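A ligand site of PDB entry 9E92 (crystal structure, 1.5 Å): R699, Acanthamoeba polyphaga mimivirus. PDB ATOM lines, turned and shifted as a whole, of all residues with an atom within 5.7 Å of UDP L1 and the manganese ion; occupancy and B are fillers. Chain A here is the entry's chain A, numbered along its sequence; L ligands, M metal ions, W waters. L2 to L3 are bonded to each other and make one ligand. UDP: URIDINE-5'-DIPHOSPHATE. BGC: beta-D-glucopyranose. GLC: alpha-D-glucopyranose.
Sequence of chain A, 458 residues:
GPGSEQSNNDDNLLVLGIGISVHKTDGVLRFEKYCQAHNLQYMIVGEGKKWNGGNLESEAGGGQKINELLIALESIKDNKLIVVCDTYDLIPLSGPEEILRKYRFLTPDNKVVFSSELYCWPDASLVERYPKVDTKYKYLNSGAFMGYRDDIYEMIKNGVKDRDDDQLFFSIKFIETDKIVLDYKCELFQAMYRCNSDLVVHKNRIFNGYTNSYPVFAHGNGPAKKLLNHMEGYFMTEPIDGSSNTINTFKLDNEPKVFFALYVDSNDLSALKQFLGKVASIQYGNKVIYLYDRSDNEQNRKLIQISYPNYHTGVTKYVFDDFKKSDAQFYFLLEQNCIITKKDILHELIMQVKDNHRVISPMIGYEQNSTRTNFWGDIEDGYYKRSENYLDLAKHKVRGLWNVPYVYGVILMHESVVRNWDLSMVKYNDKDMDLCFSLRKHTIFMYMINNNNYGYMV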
ATOM      1  N   GLY A  17      -3.683   0.636  27.085  1.00  0.00           N
ATOM      2  CA  GLY A  17      -3.587   1.797  26.224  1.00  0.00           C
ATOM      3  C   GLY A  17      -4.299   1.562  24.912  1.00  0.00           C
ATOM      4  O   GLY A  17      -3.991   0.554  24.219  1.00  0.00           O
ATOM      5  N   ILE A  18      -5.200   2.458  24.523  1.00  0.00           N
ATOM      6  CA  ILE A  18      -5.952   2.319  23.279  1.00  0.00           C
ATOM      7  C   ILE A  18      -5.105   2.782  22.083  1.00  0.00           C
ATOM      8  O   ILE A  18      -4.645   3.937  22.046  1.00  0.00           O
ATOM      9  CB  ILE A  18      -7.256   3.121  23.256  1.00  0.00           C
ATOM     10  CG1 ILE A  18      -8.099   2.891  24.496  1.00  0.00           C
ATOM     11  CG2 ILE A  18      -8.024   2.875  21.970  1.00  0.00           C
ATOM     12  CD1 ILE A  18      -8.488   1.450  24.722  1.00  0.00           C
ATOM     13  N   GLY A  19      -4.808   1.855  21.157  1.00  0.00           N
ATOM     14  CA  GLY A  19      -3.953   2.126  20.007  1.00  0.00           C
ATOM     15  C   GLY A  19      -4.441   1.345  18.773  1.00  0.00           C
ATOM     16  O   GLY A  19      -3.778   0.387  18.318  1.00  0.00           O
ATOM     17  N   ILE A  20      -5.574   1.830  18.264  1.00  0.00           N
ATOM     18  CA  ILE A  20      -6.254   1.223  17.132  1.00  0.00           C
ATOM     19  C   ILE A  20      -5.657   1.794  15.850  1.00  0.00           C
ATOM     20  O   ILE A  20      -5.966   2.911  15.448  1.00  0.00           O
ATOM     21  CB  ILE A  20      -7.751   1.499  17.233  1.00  0.00           C
ATOM     22  CG1 ILE A  20      -8.367   0.943  18.511  1.00  0.00           C
ATOM     23  CG2 ILE A  20      -8.468   0.909  16.020  1.00  0.00           C
ATOM     24  CD1 ILE A  20      -9.690   1.590  18.896  1.00  0.00           C
ATOM     25  N   SER A  21      -4.866   0.932  15.205  1.00  0.00           N
ATOM     26  CA  SER A  21      -4.179   1.278  13.961  1.00  0.00           C
ATOM     27  C   SER A  21      -3.610   0.005  13.339  1.00  0.00           C
ATOM     28  O   SER A  21      -3.068  -0.839  14.035  1.00  0.00           O
ATOM     29  CB  SER A  21      -3.043   2.267  14.297  1.00  0.00           C
ATOM     30  OG  SER A  21      -2.574   2.894  13.103  1.00  0.00           O
ATOM     31  N   VAL A  45      -4.451  -1.960  23.174  1.00  0.00           N
ATOM     32  CA  VAL A  45      -5.754  -2.453  22.707  1.00  0.00           C
ATOM     33  C   VAL A  45      -5.958  -1.997  21.266  1.00  0.00           C
ATOM     34  O   VAL A  45      -5.900  -0.810  20.945  1.00  0.00           O
ATOM     35  CB  VAL A  45      -6.867  -1.901  23.635  1.00  0.00           C
ATOM     36  CG1 VAL A  45      -8.283  -2.139  23.083  1.00  0.00           C
ATOM     37  CG2 VAL A  45      -6.685  -2.498  25.038  1.00  0.00           C
ATOM     38  N   TRP A  51      -8.907   2.384  12.441  1.00  0.00           N
ATOM     39  CA  TRP A  51      -9.749   3.312  13.194  1.00  0.00           C
ATOM     40  C   TRP A  51     -11.019   3.675  12.422  1.00  0.00           C
ATOM     41  O   TRP A  51     -10.940   4.056  11.238  1.00  0.00           O
ATOM     42  CB  TRP A  51      -8.956   4.581  13.525  1.00  0.00           C
ATOM     43  CG  TRP A  51      -9.705   5.702  14.183  1.00  0.00           C
ATOM     44  CD1 TRP A  51     -10.088   6.869  13.605  1.00  0.00           C
ATOM     45  CD2 TRP A  51     -10.071   5.829  15.577  1.00  0.00           C
ATOM     46  NE1 TRP A  51     -10.686   7.701  14.502  1.00  0.00           N
ATOM     47  CE2 TRP A  51     -10.665   7.107  15.742  1.00  0.00           C
ATOM     48  CE3 TRP A  51      -9.928   5.007  16.697  1.00  0.00           C
ATOM     49  CZ2 TRP A  51     -11.113   7.583  16.982  1.00  0.00           C
ATOM     50  CZ3 TRP A  51     -10.394   5.467  17.919  1.00  0.00           C
ATOM     51  CH2 TRP A  51     -10.956   6.730  18.050  1.00  0.00           C
ATOM     52  N   LEU A  56     -11.505  13.228  15.603  1.00  0.00           N
ATOM     53  CA  LEU A  56     -11.709  13.780  16.935  1.00  0.00           C
ATOM     54  C   LEU A  56     -11.141  15.202  17.072  1.00  0.00           C
ATOM     55  O   LEU A  56     -11.450  15.905  18.041  1.00  0.00           O
ATOM     56  CB  LEU A  56     -11.168  12.859  18.025  1.00  0.00           C
ATOM     57  CG  LEU A  56     -11.680  11.424  18.065  1.00  0.00           C
ATOM     58  CD1 LEU A  56     -11.093  10.669  19.246  1.00  0.00           C
ATOM     59  CD2 LEU A  56     -13.230  11.446  18.104  1.00  0.00           C
ATOM     60  N   LYS A  65     -13.362   3.074  20.735  1.00  0.00           N
ATOM     61  CA  LYS A  65     -12.473   2.768  21.831  1.00  0.00           C
ATOM     62  C   LYS A  65     -13.173   1.864  22.877  1.00  0.00           C
ATOM     63  O   LYS A  65     -12.557   0.930  23.368  1.00  0.00           O
ATOM     64  CB  LYS A  65     -12.034   4.091  22.497  1.00  0.00           C
ATOM     65  CG  LYS A  65     -11.251   5.056  21.648  1.00  0.00           C
ATOM     66  CD  LYS A  65     -11.223   6.476  22.230  1.00  0.00           C
ATOM     67  CE  LYS A  65     -10.588   6.560  23.544  1.00  0.00           C
ATOM     68  NZ  LYS A  65     -10.769   7.791  24.359  1.00  0.00           N
ATOM     69  N   CYS A  85      -6.386   4.167  29.026  1.00  0.00           N
ATOM     70  CA  CYS A  85      -5.993   5.522  28.645  1.00  0.00           C
ATOM     71  C   CYS A  85      -5.734   5.654  27.151  1.00  0.00           C
ATOM     72  O   CYS A  85      -5.410   4.669  26.424  1.00  0.00           O
ATOM     73  CB  CYS A  85      -4.761   5.980  29.424  1.00  0.00           C
ATOM     74  SG  CYS A  85      -3.292   4.935  29.182  1.00  0.00           S
ATOM     75  N   ASP A  86      -5.864   6.892  26.699  1.00  0.00           N
ATOM     76  CA  ASP A  86      -5.372   7.400  25.412  1.00  0.00           C
ATOM     77  C   ASP A  86      -3.873   7.110  25.297  1.00  0.00           C
ATOM     78  O   ASP A  86      -3.194   7.037  26.336  1.00  0.00           O
ATOM     79  CB  ASP A  86      -5.650   8.881  25.201  1.00  0.00           C
ATOM     80  CG  ASP A  86      -7.082   9.301  24.927  1.00  0.00           C
ATOM     81  OD1 ASP A  86      -7.962   8.350  25.015  1.00  0.00           O
ATOM     82  OD2 ASP A  86      -7.379  10.500  24.547  1.00  0.00           O
ATOM     83  N   THR A  87      -3.368   6.917  24.038  1.00  0.00           N
ATOM     84  CA  THR A  87      -1.942   6.713  23.825  1.00  0.00           C
ATOM     85  C   THR A  87      -1.305   7.725  22.872  1.00  0.00           C
ATOM     86  O   THR A  87      -0.073   7.852  22.918  1.00  0.00           O
ATOM     87  CB  THR A  87      -1.561   5.311  23.355  1.00  0.00           C
ATOM     88  OG1 THR A  87      -2.129   5.117  22.063  1.00  0.00           O
ATOM     89  CG2 THR A  87      -2.044   4.251  24.344  1.00  0.00           C
ATOM     90  N   TYR A  88      -2.081   8.392  22.016  1.00  0.00           N
ATOM     91  CA  TYR A  88      -1.496   9.160  20.935  1.00  0.00           C
ATOM     92  C   TYR A  88      -0.907  10.461  21.471  1.00  0.00           C
ATOM     93  O   TYR A  88       0.055  11.008  20.920  1.00  0.00           O
ATOM     94  CB  TYR A  88      -2.485   9.453  19.816  1.00  0.00           C
ATOM     95  CG  TYR A  88      -2.751   8.289  18.841  1.00  0.00           C
ATOM     96  CD1 TYR A  88      -2.427   6.994  19.192  1.00  0.00           C
ATOM     97  CD2 TYR A  88      -3.243   8.531  17.583  1.00  0.00           C
ATOM     98  CE1 TYR A  88      -2.672   5.914  18.338  1.00  0.00           C
ATOM     99  CE2 TYR A  88      -3.478   7.471  16.711  1.00  0.00           C
ATOM    100  CZ  TYR A  88      -3.159   6.197  17.084  1.00  0.00           C
ATOM    101  OH  TYR A  88      -3.318   5.093  16.215  1.00  0.00           O
ATOM    102  N   ASP A  89      -1.495  10.963  22.586  1.00  0.00           N
ATOM    103  CA  ASP A  89      -1.207  12.259  23.174  1.00  0.00           C
ATOM    104  C   ASP A  89      -1.031  12.176  24.703  1.00  0.00           C
ATOM    105  O   ASP A  89      -1.495  13.073  25.425  1.00  0.00           O
ATOM    106  CB  ASP A  89      -2.354  13.229  22.844  1.00  0.00           C
ATOM    107  CG  ASP A  89      -3.752  12.777  23.296  1.00  0.00           C
ATOM    108  OD1 ASP A  89      -3.874  11.648  23.799  1.00  0.00           O
ATOM    109  OD2 ASP A  89      -4.673  13.638  23.202  1.00  0.00           O
ATOM    110  N   ASN A 141     -13.191  13.781  31.830  1.00  0.00           N
ATOM    111  CA  ASN A 141     -12.437  13.481  30.614  1.00  0.00           C
ATOM    112  C   ASN A 141     -12.221  11.968  30.537  1.00  0.00           C
ATOM    113  O   ASN A 141     -11.742  11.311  31.487  1.00  0.00           O
ATOM    114  CB  ASN A 141     -11.083  14.233  30.581  1.00  0.00           C
ATOM    115  CG  ASN A 141     -10.295  13.911  29.323  1.00  0.00           C
ATOM    116  OD1 ASN A 141      -9.610  12.885  29.329  1.00  0.00           O
ATOM    117  ND2 ASN A 141     -10.404  14.729  28.298  1.00  0.00           N
ATOM    118  N   GLY A 143     -10.237  10.241  28.526  1.00  0.00           N
ATOM    119  CA  GLY A 143      -8.938   9.835  28.030  1.00  0.00           C
ATOM    120  C   GLY A 143      -8.040   9.125  29.038  1.00  0.00           C
ATOM    121  O   GLY A 143      -6.970   8.604  28.688  1.00  0.00           O
ATOM    122  N   HIS A 219      -1.629  14.175  29.825  1.00  0.00           N
ATOM    123  CA  HIS A 219      -2.495  14.035  28.668  1.00  0.00           C
ATOM    124  C   HIS A 219      -2.634  15.387  27.953  1.00  0.00           C
ATOM    125  O   HIS A 219      -3.314  16.313  28.420  1.00  0.00           O
ATOM    126  CB  HIS A 219      -3.862  13.503  29.148  1.00  0.00           C
ATOM    127  CG  HIS A 219      -4.833  13.252  28.047  1.00  0.00           C
ATOM    128  ND1 HIS A 219      -6.189  13.084  28.266  1.00  0.00           N
ATOM    129  CD2 HIS A 219      -4.654  13.088  26.648  1.00  0.00           C
ATOM    130  CE1 HIS A 219      -6.782  12.804  27.092  1.00  0.00           C
ATOM    131  NE2 HIS A 219      -5.891  12.815  26.071  1.00  0.00           N
ATOM    132  N   GLY A 220      -2.042  15.472  26.755  1.00  0.00           N
ATOM    133  CA  GLY A 220      -2.189  16.610  25.865  1.00  0.00           C
ATOM    134  C   GLY A 220      -3.460  16.546  25.066  1.00  0.00           C
ATOM    135  O   GLY A 220      -3.399  16.455  23.839  1.00  0.00           O
ATOM    136  N   ASN A 221      -4.568  16.682  25.761  1.00  0.00           N
ATOM    137  CA  ASN A 221      -5.878  16.517  25.134  1.00  0.00           C
ATOM    138  C   ASN A 221      -6.164  17.694  24.204  1.00  0.00           C
ATOM    139  O   ASN A 221      -5.720  18.843  24.380  1.00  0.00           O
ATOM    140  CB  ASN A 221      -6.977  16.304  26.164  1.00  0.00           C
ATOM    141  CG  ASN A 221      -7.223  17.479  27.074  1.00  0.00           C
ATOM    142  OD1 ASN A 221      -6.270  17.987  27.717  1.00  0.00           O
ATOM    143  ND2 ASN A 221      -8.444  18.013  27.128  1.00  0.00           N
ATOM    144  N   GLY A 222      -6.869  17.401  23.103  1.00  0.00           N
ATOM    145  CA  GLY A 222      -7.208  18.438  22.155  1.00  0.00           C
ATOM    146  C   GLY A 222      -5.951  19.125  21.603  1.00  0.00           C
ATOM    147  O   GLY A 222      -4.944  18.455  21.367  1.00  0.00           O
ATOM    148  N   PRO A 223      -5.939  20.449  21.407  1.00  0.00           N
ATOM    149  CA  PRO A 223      -4.752  21.163  20.954  1.00  0.00           C
ATOM    150  C   PRO A 223      -3.537  21.088  21.872  1.00  0.00           C
ATOM    151  O   PRO A 223      -2.445  21.456  21.434  1.00  0.00           O
ATOM    152  CB  PRO A 223      -5.239  22.626  20.770  1.00  0.00           C
ATOM    153  CG  PRO A 223      -6.741  22.459  20.636  1.00  0.00           C
ATOM    154  CD  PRO A 223      -7.139  21.311  21.476  1.00  0.00           C
ATOM    155  N   LYS A 225      -1.753  18.770  22.588  1.00  0.00           N
ATOM    156  CA  LYS A 225      -0.662  17.978  22.025  1.00  0.00           C
ATOM    157  C   LYS A 225       0.573  18.875  21.856  1.00  0.00           C
ATOM    158  O   LYS A 225       1.683  18.399  22.030  1.00  0.00           O
ATOM    159  CB  LYS A 225      -1.073  17.352  20.703  1.00  0.00           C
ATOM    160  CG  LYS A 225      -2.091  16.268  20.804  1.00  0.00           C
ATOM    161  CD  LYS A 225      -3.056  16.186  19.628  1.00  0.00           C
ATOM    162  CE  LYS A 225      -4.208  15.213  19.958  1.00  0.00           C
ATOM    163  NZ  LYS A 225      -4.932  15.588  21.164  1.00  0.00           N
HETATM  164  N1  UDP L   1      -7.117   6.552  18.693  1.00  0.00           N
HETATM  165  C2  UDP L   1      -6.698   5.339  18.177  1.00  0.00           C
HETATM  166  N3  UDP L   1      -6.510   5.341  16.804  1.00  0.00           N
HETATM  167  C4  UDP L   1      -6.736   6.402  15.955  1.00  0.00           C
HETATM  168  C5  UDP L   1      -7.211   7.610  16.562  1.00  0.00           C
HETATM  169  C6  UDP L   1      -7.421   7.638  17.901  1.00  0.00           C
HETATM  170  O2  UDP L   1      -6.430   4.394  18.896  1.00  0.00           O
HETATM  171  O4  UDP L   1      -6.487   6.271  14.736  1.00  0.00           O
HETATM  172  C1' UDP L   1      -7.246   6.563  20.205  1.00  0.00           C
HETATM  173  C2' UDP L   1      -5.909   6.940  20.887  1.00  0.00           C
HETATM  174  O2' UDP L   1      -5.721   6.281  22.141  1.00  0.00           O
HETATM  175  C3' UDP L   1      -6.062   8.432  21.055  1.00  0.00           C
HETATM  176  C4' UDP L   1      -7.534   8.498  21.487  1.00  0.00           C
HETATM  177  O4' UDP L   1      -8.149   7.572  20.546  1.00  0.00           O
HETATM  178  O3' UDP L   1      -5.109   8.937  21.994  1.00  0.00           O
HETATM  179  C5' UDP L   1      -8.232   9.814  21.468  1.00  0.00           C
HETATM  180  O5' UDP L   1      -7.869  10.608  20.343  1.00  0.00           O
HETATM  181  PA  UDP L   1      -6.809  11.789  20.634  1.00  0.00           P
HETATM  182  O1A UDP L   1      -6.033  12.029  19.370  1.00  0.00           O
HETATM  183  O2A UDP L   1      -6.107  11.432  21.892  1.00  0.00           O
HETATM  184  O3A UDP L   1      -7.684  13.037  20.935  1.00  0.00           O
HETATM  185  PB  UDP L   1      -8.278  13.915  22.096  1.00  0.00           P
HETATM  186  O1B UDP L   1      -7.828  15.225  21.727  1.00  0.00           O
HETATM  187  O2B UDP L   1      -7.900  13.322  23.482  1.00  0.00           O
HETATM  188  O3B UDP L   1      -9.720  13.615  21.653  1.00  0.00           O
HETATM  189  C2  BGC L   2     -11.053  16.095  23.604  1.00  0.00           C
HETATM  190  C3  BGC L   2     -11.618  16.923  24.790  1.00  0.00           C
HETATM  191  C4  BGC L   2     -11.766  18.405  24.452  1.00  0.00           C
HETATM  192  C5  BGC L   2     -12.556  18.484  23.131  1.00  0.00           C
HETATM  193  C6  BGC L   2     -12.687  19.880  22.599  1.00  0.00           C
HETATM  194  C1  BGC L   2     -11.909  16.274  22.342  1.00  0.00           C
HETATM  195  O1  BGC L   2     -11.463  15.498  21.234  1.00  0.00           O
HETATM  196  O2  BGC L   2     -10.941  14.692  23.887  1.00  0.00           O
HETATM  197  O3  BGC L   2     -10.784  16.792  25.946  1.00  0.00           O
HETATM  198  O4  BGC L   2     -12.450  19.114  25.516  1.00  0.00           O
HETATM  199  O5  BGC L   2     -11.901  17.683  22.106  1.00  0.00           O
HETATM  200  O6  BGC L   2     -11.391  20.454  22.442  1.00  0.00           O
HETATM  201  C1  GLC L   3     -11.827  13.925  24.833  1.00  0.00           C
HETATM  202  C2  GLC L   3     -10.983  12.775  25.297  1.00  0.00           C
HETATM  203  C3  GLC L   3     -10.818  11.652  24.278  1.00  0.00           C
HETATM  204  C4  GLC L   3     -12.201  11.216  23.824  1.00  0.00           C
HETATM  205  C5  GLC L   3     -12.926  12.446  23.252  1.00  0.00           C
HETATM  206  C6  GLC L   3     -14.337  12.107  22.770  1.00  0.00           C
HETATM  207  O2  GLC L   3      -9.704  13.328  25.729  1.00  0.00           O
HETATM  208  O3  GLC L   3     -10.181  10.507  24.834  1.00  0.00           O
HETATM  209  O4  GLC L   3     -12.112  10.156  22.896  1.00  0.00           O
HETATM  210  O5  GLC L   3     -13.050  13.481  24.225  1.00  0.00           O
HETATM  211  O6  GLC L   3     -14.960  13.207  22.134  1.00  0.00           O
HETATM  212 MN    MN M   1      -6.186  12.152  23.984  1.00  0.00          MN
HETATM  213  O   HOH W   1      -6.813   8.066  12.734  1.00  0.00           O
HETATM  214  O   HOH W   2      -3.709   5.648  13.577  1.00  0.00           O
HETATM  215  O   HOH W   3      -8.739  16.391  19.528  1.00  0.00           O
HETATM  216  O   HOH W   4      -7.242  10.792  17.033  1.00  0.00           O
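Gly 19 touches UDP L1 (CA to O2, 3.5 Å).
CB of Trp 51 touches O4 of UDP L1, at 3.2 Å.
Leu 56 touches UDP L1 (CD1 to O5', 3.4 Å).
Lys 65 touches UDP L1 (CD to O4', 3.7 Å).
C of Asn 221 touches O1B of UDP L1, at 3.9 Å.
Hydrophobic or aromatic side chains that line UDP L1: Ile 18, Ile 20, Trp 51, Leu 56, Tyr 88 and His 219.
Along chain A the residues within 4 Å of UDP L1 span positions 18 to 225.
The manganese ion is bound by the side-chain carboxylate (OD2) of Asp 86, an oxygen (O2B) of UDP L1, a ring nitrogen (NE2) of His 219, an oxygen (O2A) of UDP L1, the side-chain carboxylate (OD2) of Asp 89 and the side-chain carboxylate (OD1) of Asp 89.
The manganese ion has six donor atoms within binding distance.
Within 4 Å of the manganese ion: Asp 86, Asp 89 and His 219.
Along chain A the residues within 4 Å of the manganese ion span positions 86 to 219.
The backbone carbonyl oxygen (O) of Ile 18 sits at hydrogen-bond distance from an oxygen (O2') of UDP L1 (2.6 Å).
O1B of UDP L1 sits at hydrogen-bond distance from N of Gly 222, 2.7 Å away.
The backbone NH of Ile 20 sits at hydrogen-bond distance from an oxygen (O2) of UDP L1, 2.8 Å away.
N3 of UDP L1 lies within hydrogen-bond range of O of Ile 20, at 2.8 Å.
The side-chain amino group (NZ) of Lys 225 lies within salt-bridge range of an oxygen (O1B) of UDP L1, 3.0 Å away.
N of Tyr 88 is in hydrogen-bond range of O3' of UDP L1 (3.1 Å).
The side-chain hydroxyl of Tyr 88 lies within hydrogen-bond range of a nitrogen (N3) of UDP L1, at 3.3 Å.
N of Thr 87 lies within hydrogen-bond range of O2' of UDP L1 (3.1 Å).
OD1 of Asp 86 lies within hydrogen-bond range of O3 of GLC L3 (3.1 Å).
The backbone carbonyl oxygen (O) of Leu 56 is in hydrogen-bond range of an oxygen (O1) of BGC L2 (3.2 Å).
The side-chain amino group (NZ) of Lys 65 lies within hydrogen-bond range of an oxygen (O3) of GLC L3, at 2.8 Å.
The side-chain amide nitrogen of Asn 221 sits at hydrogen-bond distance from an oxygen (O3) of BGC L2 (2.9 Å).
The side-chain amide nitrogen of Asn 141 lies within hydrogen-bond range of an oxygen (O2) of GLC L3 (3.0 Å).
Water W3 lies within hydrogen-bond range of an oxygen (O1B) of UDP L1, the backbone carbonyl oxygen of Leu 56 and an oxygen (O1) of BGC L2.
Water W2 lies within hydrogen-bond range of OH of Tyr 88 (2.7 Å), OG of Ser 21 (3.0 Å) and O4 of UDP L1 (3.1 Å).
The backbone NH of Asp 86 lies within hydrogen-bond range of the backbone carbonyl oxygen of Gly 143.
O of His 219 lies close to OD1 of Asn 221.
The side-chain amino group (NZ) of Lys 225 lies close to the side-chain carboxylate (OD2) of Asp 89 (2.8 Å).
O of Asp 89 lies within hydrogen-bond range of N of Gly 220 (2.8 Å).
The side-chain hydroxyl (OG1) of Thr 87 sits at hydrogen-bond distance from the backbone carbonyl oxygen (O) of Ile 18 (2.8 Å).
The backbone carbonyl oxygen (O) of Cys 85 lies within hydrogen-bond range of the backbone NH (N) of Ile 18 (2.9 Å).
The side-chain amino group (NZ) of Lys 225 is in hydrogen-bond range of the backbone carbonyl oxygen (O) of Gly 222 (2.9 Å).
The backbone NH (N) of Gly 19 lies within hydrogen-bond range of the backbone carbonyl oxygen (O) of Val 45 (2.9 Å).
An oxygen (O1) of BGC L2 is in hydrogen-bond range of an oxygen (O3B) of UDP L1 (2.6 Å).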
